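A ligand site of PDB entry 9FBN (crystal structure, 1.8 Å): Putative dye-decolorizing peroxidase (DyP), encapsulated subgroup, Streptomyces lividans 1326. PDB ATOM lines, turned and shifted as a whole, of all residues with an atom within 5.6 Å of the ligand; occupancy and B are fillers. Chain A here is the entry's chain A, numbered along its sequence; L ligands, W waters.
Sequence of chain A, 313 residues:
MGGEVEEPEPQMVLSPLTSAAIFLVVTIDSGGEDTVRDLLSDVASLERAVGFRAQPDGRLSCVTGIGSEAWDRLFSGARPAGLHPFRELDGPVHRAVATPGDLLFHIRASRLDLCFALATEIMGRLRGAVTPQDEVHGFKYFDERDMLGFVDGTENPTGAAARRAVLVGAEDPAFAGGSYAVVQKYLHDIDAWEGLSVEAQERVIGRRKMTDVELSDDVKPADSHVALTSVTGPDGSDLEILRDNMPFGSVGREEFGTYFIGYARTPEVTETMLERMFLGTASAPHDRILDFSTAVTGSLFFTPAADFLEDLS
The backbone NH of Glu 155 sits at hydrogen-bond distance from an oxygen (O2) of the ligand (2.9 Å). NE2 of His 225 binds FE1 of the ligand (2.1 Å). An oxygen (O1) of the ligand lies within salt-bridge range of the guanidinium group (NH1) of Arg 243. N of Gly 153 lies within hydrogen-bond range of O1 of the ligand.
Water W1 bridges an oxygen (O3) of the ligand (2.8 Å) and the backbone carbonyl oxygen of Thr 229 (3.0 Å). Water W2 bridges the guanidinium group (NH1) of Arg 207 (2.7 Å) and an oxygen (O4) of the ligand (2.8 Å).
The backbone carbonyl oxygen (O) of His 225 lies within hydrogen-bond range of the side-chain hydroxyl (OG1) of Thr 229, 2.9 Å away. N of Tyr 186 lies within hydrogen-bond range of O of Thr 258, 3.0 Å away. The side-chain hydroxyl (OG) of Ser 230 lies within hydrogen-bond range of the backbone carbonyl oxygen (O) of Val 226, at 2.5 Å. The backbone carbonyl oxygen of Ile 289 is in hydrogen-bond range of the side-chain hydroxyl of Ser 293. The guanidinium group (NH1) of Arg 207 is in salt-bridge range of the side-chain carboxylate (OE1) of Glu 214 (3.96 Å). The side-chain carboxylate (OD2) of Asp 152 lies close to the side-chain carboxylate (OD2) of Asp 146 (2.6 Å). A ring nitrogen (NE2) of His 188 is in hydrogen-bond range of the side-chain hydroxyl of Thr 258 (2.9 Å). The guanidinium group (NH1) of Arg 243 is in salt-bridge range of the side-chain carboxylate (OD1) of Asp 152 (3.7 Å).
Asp 146 touches the ligand (OD2 to C9, 3.6 Å). Phe 150 touches the ligand (CB to C9, 3.99 Å). O of Val 151 touches C9 of the ligand (3.3 Å). Asp 152 touches the ligand. N of Thr 154 touches C12 of the ligand, at 3.4 Å. OE1 of Gln 184 touches C24 of the ligand (3.3 Å). CG of Tyr 186 touches C19 of the ligand, at 3.6 Å. Arg 207 touches the ligand (CD to C10, 3.5 Å). CG1 of Val 226 touches O4 of the ligand, at 3.8 Å. Thr 229 touches the ligand. OG of Ser 230 touches O3 of the ligand (3.9 Å). Asn 245 touches the ligand. Thr 258 touches the ligand. Phe 260 touches the ligand (CE1 to C22, 3.5 Å). CE of Met 273 touches C31 of the ligand (3.8 Å). CD2 of Leu 274 touches C26 of the ligand (3.7 Å). Met 277 touches the ligand (SD to C21, 3.8 Å). Ile 289 touches the ligand. 22 residues have an atom within 4 Å of the ligand: Asp 146, Phe 150, Val 151, Asp 152, Gly 153, Thr 154, Glu 155, Gln 184, Tyr 186, Arg 207, His 225, Val 226, Thr 229, Ser 230, Arg 243, Asn 245, Thr 258, Phe 260, Met 273, Leu 274, Met 277 and Ile 289. The nearest printed residue that does not touch the ligand is Thr 270 (4.01 Å).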
ATOM      1  N   ASP A 146      13.552   6.170  16.518  1.00  0.00           N
ATOM      2  CA  ASP A 146      13.745   4.782  16.134  1.00  0.00           C
ATOM      3  C   ASP A 146      15.104   4.355  16.710  1.00  0.00           C
ATOM      4  O   ASP A 146      15.821   5.166  17.308  1.00  0.00           O
ATOM      5  CB  ASP A 146      13.518   4.623  14.658  1.00  0.00           C
ATOM      6  CG  ASP A 146      14.432   5.490  13.803  1.00  0.00           C
ATOM      7  OD1 ASP A 146      15.555   5.794  14.245  1.00  0.00           O
ATOM      8  OD2 ASP A 146      13.962   5.919  12.712  1.00  0.00           O
ATOM      9  N   LEU A 148      17.813   3.958  15.218  1.00  0.00           N
ATOM     10  CA  LEU A 148      18.916   4.714  14.653  1.00  0.00           C
ATOM     11  C   LEU A 148      19.075   6.081  15.354  1.00  0.00           C
ATOM     12  O   LEU A 148      20.041   6.829  15.143  1.00  0.00           O
ATOM     13  CB  LEU A 148      18.717   4.869  13.157  1.00  0.00           C
ATOM     14  CG  LEU A 148      18.640   3.634  12.251  1.00  0.00           C
ATOM     15  CD1 LEU A 148      18.602   4.117  10.860  1.00  0.00           C
ATOM     16  CD2 LEU A 148      19.822   2.723  12.418  1.00  0.00           C
ATOM     17  N   PHE A 150      16.889   8.664  15.390  1.00  0.00           N
ATOM     18  CA  PHE A 150      16.149   9.784  14.790  1.00  0.00           C
ATOM     19  C   PHE A 150      14.675   9.718  15.178  1.00  0.00           C
ATOM     20  O   PHE A 150      14.043   8.680  15.230  1.00  0.00           O
ATOM     21  CB  PHE A 150      16.404   9.810  13.279  1.00  0.00           C
ATOM     22  CG  PHE A 150      17.759  10.292  12.825  1.00  0.00           C
ATOM     23  CD1 PHE A 150      18.951   9.558  13.137  1.00  0.00           C
ATOM     24  CD2 PHE A 150      17.900  11.560  12.250  1.00  0.00           C
ATOM     25  CE1 PHE A 150      20.207  10.095  12.787  1.00  0.00           C
ATOM     26  CE2 PHE A 150      19.112  12.022  11.809  1.00  0.00           C
ATOM     27  CZ  PHE A 150      20.300  11.301  12.118  1.00  0.00           C
ATOM     28  N   VAL A 151      14.045  10.878  15.145  1.00  0.00           N
ATOM     29  CA  VAL A 151      12.581  10.956  15.220  1.00  0.00           C
ATOM     30  C   VAL A 151      11.949  10.315  13.988  1.00  0.00           C
ATOM     31  O   VAL A 151      12.476  10.421  12.876  1.00  0.00           O
ATOM     32  CB  VAL A 151      12.097  12.407  15.425  1.00  0.00           C
ATOM     33  CG1 VAL A 151      10.547  12.428  15.513  1.00  0.00           C
ATOM     34  CG2 VAL A 151      12.734  13.120  16.639  1.00  0.00           C
ATOM     35  N   ASP A 152      10.839   9.612  14.154  1.00  0.00           N
ATOM     36  CA  ASP A 152      10.365   8.686  13.125  1.00  0.00           C
ATOM     37  C   ASP A 152       8.846   8.843  13.070  1.00  0.00           C
ATOM     38  O   ASP A 152       8.173   8.591  14.093  1.00  0.00           O
ATOM     39  CB  ASP A 152      10.824   7.266  13.349  1.00  0.00           C
ATOM     40  CG  ASP A 152      10.633   6.328  12.184  1.00  0.00           C
ATOM     41  OD1 ASP A 152       9.598   6.425  11.548  1.00  0.00           O
ATOM     42  OD2 ASP A 152      11.544   5.475  11.945  1.00  0.00           O
ATOM     43  N   GLY A 153       8.387   9.543  12.007  1.00  0.00           N
ATOM     44  CA  GLY A 153       6.950   9.743  11.744  1.00  0.00           C
ATOM     45  C   GLY A 153       6.567  11.189  11.512  1.00  0.00           C
ATOM     46  O   GLY A 153       5.384  11.511  11.229  1.00  0.00           O
ATOM     47  N   THR A 154       7.569  12.103  11.581  1.00  0.00           N
ATOM     48  CA  THR A 154       7.337  13.543  11.509  1.00  0.00           C
ATOM     49  C   THR A 154       6.536  14.010  10.296  1.00  0.00           C
ATOM     50  O   THR A 154       5.620  14.807  10.505  1.00  0.00           O
ATOM     51  CB  THR A 154       8.673  14.278  11.531  1.00  0.00           C
ATOM     52  OG1 THR A 154       9.432  13.715  12.605  1.00  0.00           O
ATOM     53  CG2 THR A 154       8.481  15.785  11.655  1.00  0.00           C
ATOM     54  N   GLU A 155       6.868  13.562   9.049  1.00  0.00           N
ATOM     55  CA  GLU A 155       6.188  14.128   7.895  1.00  0.00           C
ATOM     56  C   GLU A 155       5.039  13.227   7.392  1.00  0.00           C
ATOM     57  O   GLU A 155       4.527  13.465   6.279  1.00  0.00           O
ATOM     58  CB  GLU A 155       7.165  14.301   6.700  1.00  0.00           C
ATOM     59  CG  GLU A 155       8.177  15.410   6.891  1.00  0.00           C
ATOM     60  CD  GLU A 155       7.495  16.753   6.997  1.00  0.00           C
ATOM     61  OE1 GLU A 155       6.818  17.009   6.051  1.00  0.00           O
ATOM     62  OE2 GLU A 155       7.454  17.407   8.023  1.00  0.00           O
ATOM     63  N   ASN A 156       4.554  12.313   8.230  1.00  0.00           N
ATOM     64  CA  ASN A 156       3.286  11.610   8.050  1.00  0.00           C
ATOM     65  C   ASN A 156       2.121  12.602   7.789  1.00  0.00           C
ATOM     66  O   ASN A 156       2.013  13.666   8.387  1.00  0.00           O
ATOM     67  CB  ASN A 156       2.830  10.783   9.246  1.00  0.00           C
ATOM     68  CG  ASN A 156       3.214   9.317   9.119  1.00  0.00           C
ATOM     69  OD1 ASN A 156       3.326   8.795   8.012  1.00  0.00           O
ATOM     70  ND2 ASN A 156       3.589   8.671  10.199  1.00  0.00           N
ATOM     71  N   GLN A 184       7.633  -4.638   6.099  1.00  0.00           N
ATOM     72  CA  GLN A 184       8.963  -5.207   6.028  1.00  0.00           C
ATOM     73  C   GLN A 184       9.587  -5.128   7.417  1.00  0.00           C
ATOM     74  O   GLN A 184       9.677  -4.053   7.991  1.00  0.00           O
ATOM     75  CB  GLN A 184       9.952  -4.565   5.059  1.00  0.00           C
ATOM     76  CG  GLN A 184       9.507  -4.349   3.606  1.00  0.00           C
ATOM     77  CD  GLN A 184      10.471  -3.444   2.882  1.00  0.00           C
ATOM     78  OE1 GLN A 184      10.474  -2.212   3.055  1.00  0.00           O
ATOM     79  NE2 GLN A 184      11.326  -4.048   2.098  1.00  0.00           N
ATOM     80  N   TYR A 186      13.004  -4.879   9.345  1.00  0.00           N
ATOM     81  CA  TYR A 186      14.387  -4.504   9.074  1.00  0.00           C
ATOM     82  C   TYR A 186      15.239  -4.741  10.316  1.00  0.00           C
ATOM     83  O   TYR A 186      14.760  -4.445  11.425  1.00  0.00           O
ATOM     84  CB  TYR A 186      14.604  -3.021   8.749  1.00  0.00           C
ATOM     85  CG  TYR A 186      14.146  -2.574   7.342  1.00  0.00           C
ATOM     86  CD1 TYR A 186      15.042  -2.700   6.264  1.00  0.00           C
ATOM     87  CD2 TYR A 186      12.841  -2.199   7.028  1.00  0.00           C
ATOM     88  CE1 TYR A 186      14.697  -2.354   4.977  1.00  0.00           C
ATOM     89  CE2 TYR A 186      12.498  -1.809   5.744  1.00  0.00           C
ATOM     90  CZ  TYR A 186      13.422  -1.924   4.697  1.00  0.00           C
ATOM     91  OH  TYR A 186      13.208  -1.512   3.379  1.00  0.00           O
ATOM     92  N   HIS A 188      19.001  -3.650  11.888  1.00  0.00           N
ATOM     93  CA  HIS A 188      20.066  -2.670  11.737  1.00  0.00           C
ATOM     94  C   HIS A 188      21.435  -3.122  12.272  1.00  0.00           C
ATOM     95  O   HIS A 188      21.565  -3.770  13.310  1.00  0.00           O
ATOM     96  CB  HIS A 188      19.710  -1.435  12.536  1.00  0.00           C
ATOM     97  CG  HIS A 188      18.465  -0.782  12.055  1.00  0.00           C
ATOM     98  ND1 HIS A 188      18.385  -0.302  10.768  1.00  0.00           N
ATOM     99  CD2 HIS A 188      17.280  -0.561  12.644  1.00  0.00           C
ATOM    100  CE1 HIS A 188      17.189   0.257  10.580  1.00  0.00           C
ATOM    101  NE2 HIS A 188      16.474   0.096  11.697  1.00  0.00           N
ATOM    102  N   ILE A 205      20.120  10.303   6.504  1.00  0.00           N
ATOM    103  CA  ILE A 205      18.694  10.367   6.676  1.00  0.00           C
ATOM    104  C   ILE A 205      18.102  11.528   5.888  1.00  0.00           C
ATOM    105  O   ILE A 205      17.016  11.398   5.355  1.00  0.00           O
ATOM    106  CB  ILE A 205      18.325  10.532   8.178  1.00  0.00           C
ATOM    107  CG1 ILE A 205      18.880   9.424   9.099  1.00  0.00           C
ATOM    108  CG2 ILE A 205      16.871  10.799   8.326  1.00  0.00           C
ATOM    109  CD1 ILE A 205      18.264   8.070   8.804  1.00  0.00           C
ATOM    110  N   ARG A 207      17.785  14.872   7.656  1.00  0.00           N
ATOM    111  CA  ARG A 207      17.257  15.695   8.724  1.00  0.00           C
ATOM    112  C   ARG A 207      18.277  15.790   9.873  1.00  0.00           C
ATOM    113  O   ARG A 207      19.077  14.870  10.099  1.00  0.00           O
ATOM    114  CB  ARG A 207      15.953  15.122   9.281  1.00  0.00           C
ATOM    115  CG  ARG A 207      14.769  14.787   8.353  1.00  0.00           C
ATOM    116  CD  ARG A 207      13.481  14.312   9.008  1.00  0.00           C
ATOM    117  NE  ARG A 207      12.803  15.455   9.579  1.00  0.00           N
ATOM    118  CZ  ARG A 207      11.855  16.192   8.997  1.00  0.00           C
ATOM    119  NH1 ARG A 207      11.497  15.974   7.707  1.00  0.00           N
ATOM    120  NH2 ARG A 207      11.420  17.234   9.617  1.00  0.00           N
ATOM    121  N   ASP A 212      15.354  17.487  14.566  1.00  0.00           N
ATOM    122  CA  ASP A 212      14.407  16.957  13.597  1.00  0.00           C
ATOM    123  C   ASP A 212      14.045  17.983  12.524  1.00  0.00           C
ATOM    124  O   ASP A 212      12.976  17.898  11.968  1.00  0.00           O
ATOM    125  CB  ASP A 212      13.175  16.408  14.298  1.00  0.00           C
ATOM    126  CG  ASP A 212      12.444  15.413  13.409  1.00  0.00           C
ATOM    127  OD1 ASP A 212      13.082  14.978  12.438  1.00  0.00           O
ATOM    128  OD2 ASP A 212      11.256  15.191  13.574  1.00  0.00           O
ATOM    129  N   GLU A 214      14.412  19.477   8.853  1.00  0.00           N
ATOM    130  CA  GLU A 214      14.817  19.122   7.502  1.00  0.00           C
ATOM    131  C   GLU A 214      16.085  19.830   7.033  1.00  0.00           C
ATOM    132  O   GLU A 214      16.302  21.010   7.286  1.00  0.00           O
ATOM    133  CB  GLU A 214      13.650  19.282   6.504  1.00  0.00           C
ATOM    134  CG  GLU A 214      13.904  18.473   5.242  1.00  0.00           C
ATOM    135  CD  GLU A 214      12.764  18.284   4.227  1.00  0.00           C
ATOM    136  OE1 GLU A 214      11.624  18.402   4.579  1.00  0.00           O
ATOM    137  OE2 GLU A 214      13.067  17.989   3.074  1.00  0.00           O
ATOM    138  N   HIS A 225      17.697   9.421   2.683  1.00  0.00           N
ATOM    139  CA  HIS A 225      16.448   8.719   2.792  1.00  0.00           C
ATOM    140  C   HIS A 225      15.278   9.603   2.344  1.00  0.00           C
ATOM    141  O   HIS A 225      14.357   9.140   1.658  1.00  0.00           O
ATOM    142  CB  HIS A 225      16.242   8.115   4.185  1.00  0.00           C
ATOM    143  CG  HIS A 225      15.006   7.302   4.371  1.00  0.00           C
ATOM    144  ND1 HIS A 225      14.704   6.224   3.573  1.00  0.00           N
ATOM    145  CD2 HIS A 225      13.968   7.370   5.294  1.00  0.00           C
ATOM    146  CE1 HIS A 225      13.592   5.613   4.088  1.00  0.00           C
ATOM    147  NE2 HIS A 225      13.023   6.339   5.018  1.00  0.00           N
ATOM    148  N   VAL A 226      15.308  10.831   2.810  1.00  0.00           N
ATOM    149  CA  VAL A 226      14.191  11.745   2.650  1.00  0.00           C
ATOM    150  C   VAL A 226      14.090  12.157   1.179  1.00  0.00           C
ATOM    151  O   VAL A 226      13.016  12.486   0.693  1.00  0.00           O
ATOM    152  CB  VAL A 226      14.325  12.991   3.583  1.00  0.00           C
ATOM    153  CG1 VAL A 226      13.484  14.209   3.135  1.00  0.00           C
ATOM    154  CG2 VAL A 226      13.952  12.661   5.030  1.00  0.00           C
ATOM    155  N   THR A 229      12.543   9.131  -0.808  1.00  0.00           N
ATOM    156  CA  THR A 229      11.183   8.711  -0.535  1.00  0.00           C
ATOM    157  C   THR A 229      10.246   9.924  -0.734  1.00  0.00           C
ATOM    158  O   THR A 229       9.091   9.821  -0.352  1.00  0.00           O
ATOM    159  CB  THR A 229      11.078   8.135   0.878  1.00  0.00           C
ATOM    160  OG1 THR A 229      11.452   9.199   1.760  1.00  0.00           O
ATOM    161  CG2 THR A 229      11.929   6.928   1.176  1.00  0.00           C
ATOM    162  N   SER A 230      10.746  11.085  -1.194  1.00  0.00           N
ATOM    163  CA  SER A 230       9.899  12.212  -1.601  1.00  0.00           C
ATOM    164  C   SER A 230       9.561  12.068  -3.078  1.00  0.00           C
ATOM    165  O   SER A 230      10.447  12.158  -3.964  1.00  0.00           O
ATOM    166  CB  SER A 230      10.509  13.574  -1.393  1.00  0.00           C
ATOM    167  OG  SER A 230      10.983  13.695  -0.066  1.00  0.00           O
ATOM    168  N   ILE A 241       2.342   8.442   1.836  1.00  0.00           N
ATOM    169  CA  ILE A 241       1.927   7.212   2.495  1.00  0.00           C
ATOM    170  C   ILE A 241       1.828   7.533   3.988  1.00  0.00           C
ATOM    171  O   ILE A 241       2.330   8.567   4.474  1.00  0.00           O
ATOM    172  CB  ILE A 241       2.848   5.995   2.167  1.00  0.00           C
ATOM    173  CG1 ILE A 241       4.205   6.183   2.822  1.00  0.00           C
ATOM    174  CG2 ILE A 241       2.988   5.719   0.654  1.00  0.00           C
ATOM    175  CD1 ILE A 241       5.061   4.934   2.858  1.00  0.00           C
ATOM    176  N   ARG A 243       2.797   5.934   7.630  1.00  0.00           N
ATOM    177  CA  ARG A 243       3.674   4.973   8.326  1.00  0.00           C
ATOM    178  C   ARG A 243       3.353   4.922   9.828  1.00  0.00           C
ATOM    179  O   ARG A 243       3.002   5.916  10.479  1.00  0.00           O
ATOM    180  CB  ARG A 243       5.136   5.426   8.098  1.00  0.00           C
ATOM    181  CG  ARG A 243       5.577   5.335   6.623  1.00  0.00           C
ATOM    182  CD  ARG A 243       6.832   6.106   6.364  1.00  0.00           C
ATOM    183  NE  ARG A 243       6.705   7.547   6.637  1.00  0.00           N
ATOM    184  CZ  ARG A 243       7.403   8.247   7.531  1.00  0.00           C
ATOM    185  NH1 ARG A 243       8.330   7.746   8.323  1.00  0.00           N
ATOM    186  NH2 ARG A 243       7.189   9.504   7.645  1.00  0.00           N
ATOM    187  N   ASN A 245       5.969   3.009  11.876  1.00  0.00           N
ATOM    188  CA  ASN A 245       7.178   2.244  12.151  1.00  0.00           C
ATOM    189  C   ASN A 245       7.397   2.061  13.671  1.00  0.00           C
ATOM    190  O   ASN A 245       7.280   3.003  14.476  1.00  0.00           O
ATOM    191  CB  ASN A 245       8.399   2.964  11.639  1.00  0.00           C
ATOM    192  CG  ASN A 245       8.424   3.177  10.150  1.00  0.00           C
ATOM    193  OD1 ASN A 245       7.560   2.652   9.439  1.00  0.00           O
ATOM    194  ND2 ASN A 245       9.442   3.890   9.695  1.00  0.00           N
ATOM    195  N   THR A 258      13.764  -2.156  13.153  1.00  0.00           N
ATOM    196  CA  THR A 258      12.595  -1.319  12.848  1.00  0.00           C
ATOM    197  C   THR A 258      11.578  -2.198  12.097  1.00  0.00           C
ATOM    198  O   THR A 258      11.887  -2.735  11.049  1.00  0.00           O
ATOM    199  CB  THR A 258      12.969  -0.099  12.030  1.00  0.00           C
ATOM    200  OG1 THR A 258      13.881   0.758  12.711  1.00  0.00           O
ATOM    201  CG2 THR A 258      11.732   0.711  11.655  1.00  0.00           C
ATOM    202  N   PHE A 260       8.715  -1.828   9.728  1.00  0.00           N
ATOM    203  CA  PHE A 260       8.135  -0.856   8.834  1.00  0.00           C
ATOM    204  C   PHE A 260       6.721  -1.288   8.482  1.00  0.00           C
ATOM    205  O   PHE A 260       6.515  -2.459   8.116  1.00  0.00           O
ATOM    206  CB  PHE A 260       8.957  -0.724   7.522  1.00  0.00           C
ATOM    207  CG  PHE A 260       8.200   0.090   6.446  1.00  0.00           C
ATOM    208  CD1 PHE A 260       8.171   1.478   6.470  1.00  0.00           C
ATOM    209  CD2 PHE A 260       7.602  -0.513   5.369  1.00  0.00           C
ATOM    210  CE1 PHE A 260       7.453   2.206   5.500  1.00  0.00           C
ATOM    211  CE2 PHE A 260       6.913   0.233   4.371  1.00  0.00           C
ATOM    212  CZ  PHE A 260       6.872   1.560   4.457  1.00  0.00           C
ATOM    213  N   THR A 270       3.611   3.145  -2.663  1.00  0.00           N
ATOM    214  CA  THR A 270       4.635   2.485  -1.825  1.00  0.00           C
ATOM    215  C   THR A 270       5.724   1.790  -2.685  1.00  0.00           C
ATOM    216  O   THR A 270       6.935   1.884  -2.383  1.00  0.00           O
ATOM    217  CB  THR A 270       3.906   1.561  -0.873  1.00  0.00           C
ATOM    218  OG1 THR A 270       2.852   2.342  -0.359  1.00  0.00           O
ATOM    219  CG2 THR A 270       4.773   0.977   0.224  1.00  0.00           C
ATOM    220  N   MET A 273       8.333   4.137  -4.120  1.00  0.00           N
ATOM    221  CA  MET A 273       9.368   4.549  -3.156  1.00  0.00           C
ATOM    222  C   MET A 273      10.341   3.425  -2.858  1.00  0.00           C
ATOM    223  O   MET A 273      11.515   3.691  -2.683  1.00  0.00           O
ATOM    224  CB  MET A 273       8.751   4.967  -1.812  1.00  0.00           C
ATOM    225  CG  MET A 273       7.918   6.250  -1.807  1.00  0.00           C
ATOM    226  SD  MET A 273       6.889   6.341  -0.303  1.00  0.00           S
ATOM    227  CE  MET A 273       6.021   7.894  -0.517  1.00  0.00           C
ATOM    228  N   LEU A 274       9.886   2.157  -2.936  1.00  0.00           N
ATOM    229  CA  LEU A 274      10.750   1.028  -2.686  1.00  0.00           C
ATOM    230  C   LEU A 274      11.694   0.928  -3.876  1.00  0.00           C
ATOM    231  O   LEU A 274      12.811   0.515  -3.712  1.00  0.00           O
ATOM    232  CB  LEU A 274      10.026  -0.306  -2.477  1.00  0.00           C
ATOM    233  CG  LEU A 274       9.232  -0.497  -1.161  1.00  0.00           C
ATOM    234  CD1 LEU A 274       8.208  -1.639  -1.133  1.00  0.00           C
ATOM    235  CD2 LEU A 274      10.248  -0.745  -0.038  1.00  0.00           C
ATOM    236  N   MET A 277      14.542   3.348  -3.518  1.00  0.00           N
ATOM    237  CA  MET A 277      15.464   2.940  -2.475  1.00  0.00           C
ATOM    238  C   MET A 277      16.418   1.835  -2.909  1.00  0.00           C
ATOM    239  O   MET A 277      17.633   1.887  -2.593  1.00  0.00           O
ATOM    240  CB  MET A 277      14.670   2.496  -1.227  1.00  0.00           C
ATOM    241  CG  MET A 277      13.946   3.611  -0.507  1.00  0.00           C
ATOM    242  SD  MET A 277      12.920   3.102   0.909  1.00  0.00           S
ATOM    243  CE  MET A 277      14.274   2.346   1.832  1.00  0.00           C
ATOM    244  N   ILE A 289      20.299   4.642   3.731  1.00  0.00           N
ATOM    245  CA  ILE A 289      19.777   3.959   4.923  1.00  0.00           C
ATOM    246  C   ILE A 289      19.891   2.431   4.794  1.00  0.00           C
ATOM    247  O   ILE A 289      20.129   1.750   5.820  1.00  0.00           O
ATOM    248  CB  ILE A 289      18.348   4.394   5.225  1.00  0.00           C
ATOM    249  CG1 ILE A 289      18.086   4.323   6.742  1.00  0.00           C
ATOM    250  CG2 ILE A 289      17.309   3.582   4.473  1.00  0.00           C
ATOM    251  CD1 ILE A 289      16.816   5.003   7.193  1.00  0.00           C
ATOM    252  N   LEU A 290      19.935   1.895   3.546  1.00  0.00           N
ATOM    253  CA  LEU A 290      20.044   0.427   3.380  1.00  0.00           C
ATOM    254  C   LEU A 290      21.460  -0.121   3.618  1.00  0.00           C
ATOM    255  O   LEU A 290      21.648  -1.345   3.788  1.00  0.00           O
ATOM    256  CB  LEU A 290      19.540   0.013   2.011  1.00  0.00           C
ATOM    257  CG  LEU A 290      18.075   0.345   1.734  1.00  0.00           C
ATOM    258  CD1 LEU A 290      17.809   0.076   0.228  1.00  0.00           C
ATOM    259  CD2 LEU A 290      17.119  -0.454   2.683  1.00  0.00           C
ATOM    260  N   SER A 293      20.783  -1.220   7.096  1.00  0.00           N
ATOM    261  CA  SER A 293      19.503  -1.839   7.379  1.00  0.00           C
ATOM    262  C   SER A 293      19.265  -2.945   6.370  1.00  0.00           C
ATOM    263  O   SER A 293      19.421  -2.737   5.136  1.00  0.00           O
ATOM    264  CB  SER A 293      18.346  -0.855   7.375  1.00  0.00           C
ATOM    265  OG  SER A 293      18.674   0.313   8.074  1.00  0.00           O
HETATM  266  C1  LIG L   1      10.862   9.254   6.449  1.00  0.00           C
HETATM  267  C2  LIG L   1      13.242   6.056   9.116  1.00  0.00           C
HETATM  268  C3  LIG L   1      11.991   2.748   5.876  1.00  0.00           C
HETATM  269  C4  LIG L   1       9.223   5.784   3.606  1.00  0.00           C
HETATM  270  C5  LIG L   1      11.675   8.721   7.428  1.00  0.00           C
HETATM  271  C6  LIG L   1      12.287   9.414   8.492  1.00  0.00           C
HETATM  272  C7  LIG L   1      12.993   8.501   9.208  1.00  0.00           C
HETATM  273  C8  LIG L   1      12.665   7.237   8.663  1.00  0.00           C
HETATM  274  C9  LIG L   1      13.852   8.682  10.421  1.00  0.00           C
HETATM  275  C10 LIG L   1      12.318  10.986   8.779  1.00  0.00           C
HETATM  276  C11 LIG L   1      11.162  11.463   9.732  1.00  0.00           C
HETATM  277  C12 LIG L   1       9.811  11.195   9.175  1.00  0.00           C
HETATM  278  O1  LIG L   1       9.319  10.028   9.363  1.00  0.00           O
HETATM  279  O2  LIG L   1       9.247  12.040   8.443  1.00  0.00           O
HETATM  280  C13 LIG L   1      13.072   4.837   8.497  1.00  0.00           C
HETATM  281  C14 LIG L   1      13.719   3.645   8.852  1.00  0.00           C
HETATM  282  C15 LIG L   1      13.343   2.661   7.971  1.00  0.00           C
HETATM  283  C16 LIG L   1      12.510   3.343   6.984  1.00  0.00           C
HETATM  284  C17 LIG L   1      14.478   3.313  10.162  1.00  0.00           C
HETATM  285  C18 LIG L   1      13.921   1.293   8.084  1.00  0.00           C
HETATM  286  C19 LIG L   1      14.720   0.927   7.102  1.00  0.00           C
HETATM  287  C20 LIG L   1      11.141   3.249   4.943  1.00  0.00           C
HETATM  288  C21 LIG L   1      10.548   2.570   3.844  1.00  0.00           C
HETATM  289  C22 LIG L   1       9.717   3.443   3.176  1.00  0.00           C
HETATM  290  C23 LIG L   1       9.872   4.685   3.883  1.00  0.00           C
HETATM  291  C24 LIG L   1      10.700   1.084   3.465  1.00  0.00           C
HETATM  292  C25 LIG L   1       8.870   3.330   1.950  1.00  0.00           C
HETATM  293  C26 LIG L   1       8.538   2.296   1.265  1.00  0.00           C
HETATM  294  C27 LIG L   1       9.539   7.016   4.263  1.00  0.00           C
HETATM  295  C28 LIG L   1       8.829   8.272   3.904  1.00  0.00           C
HETATM  296  C29 LIG L   1       9.267   9.244   4.634  1.00  0.00           C
HETATM  297  C30 LIG L   1      10.279   8.538   5.487  1.00  0.00           C
HETATM  298  C31 LIG L   1       7.768   8.417   2.808  1.00  0.00           C
HETATM  299  C32 LIG L   1       8.896  10.717   4.686  1.00  0.00           C
HETATM  300  C33 LIG L   1       9.680  11.530   3.683  1.00  0.00           C
HETATM  301  C34 LIG L   1       9.266  12.995   3.539  1.00  0.00           C
HETATM  302  O3  LIG L   1       8.348  13.334   2.736  1.00  0.00           O
HETATM  303  O4  LIG L   1       9.823  13.895   4.117  1.00  0.00           O
HETATM  304  N1  LIG L   1      11.939   7.426   7.430  1.00  0.00           N
HETATM  305  N2  LIG L   1      12.512   4.632   7.302  1.00  0.00           N
HETATM  306  N3  LIG L   1      10.683   4.476   5.026  1.00  0.00           N
HETATM  307  N4  LIG L   1      10.316   7.233   5.303  1.00  0.00           N
HETATM  308 FE1  LIG L   1      11.392   5.975   6.253  1.00  0.00          FE
HETATM  309  O   HOH W   1       7.042  11.403   1.196  1.00  0.00           O
HETATM  310  O   HOH W   2      11.079  13.526   6.644  1.00  0.00           O
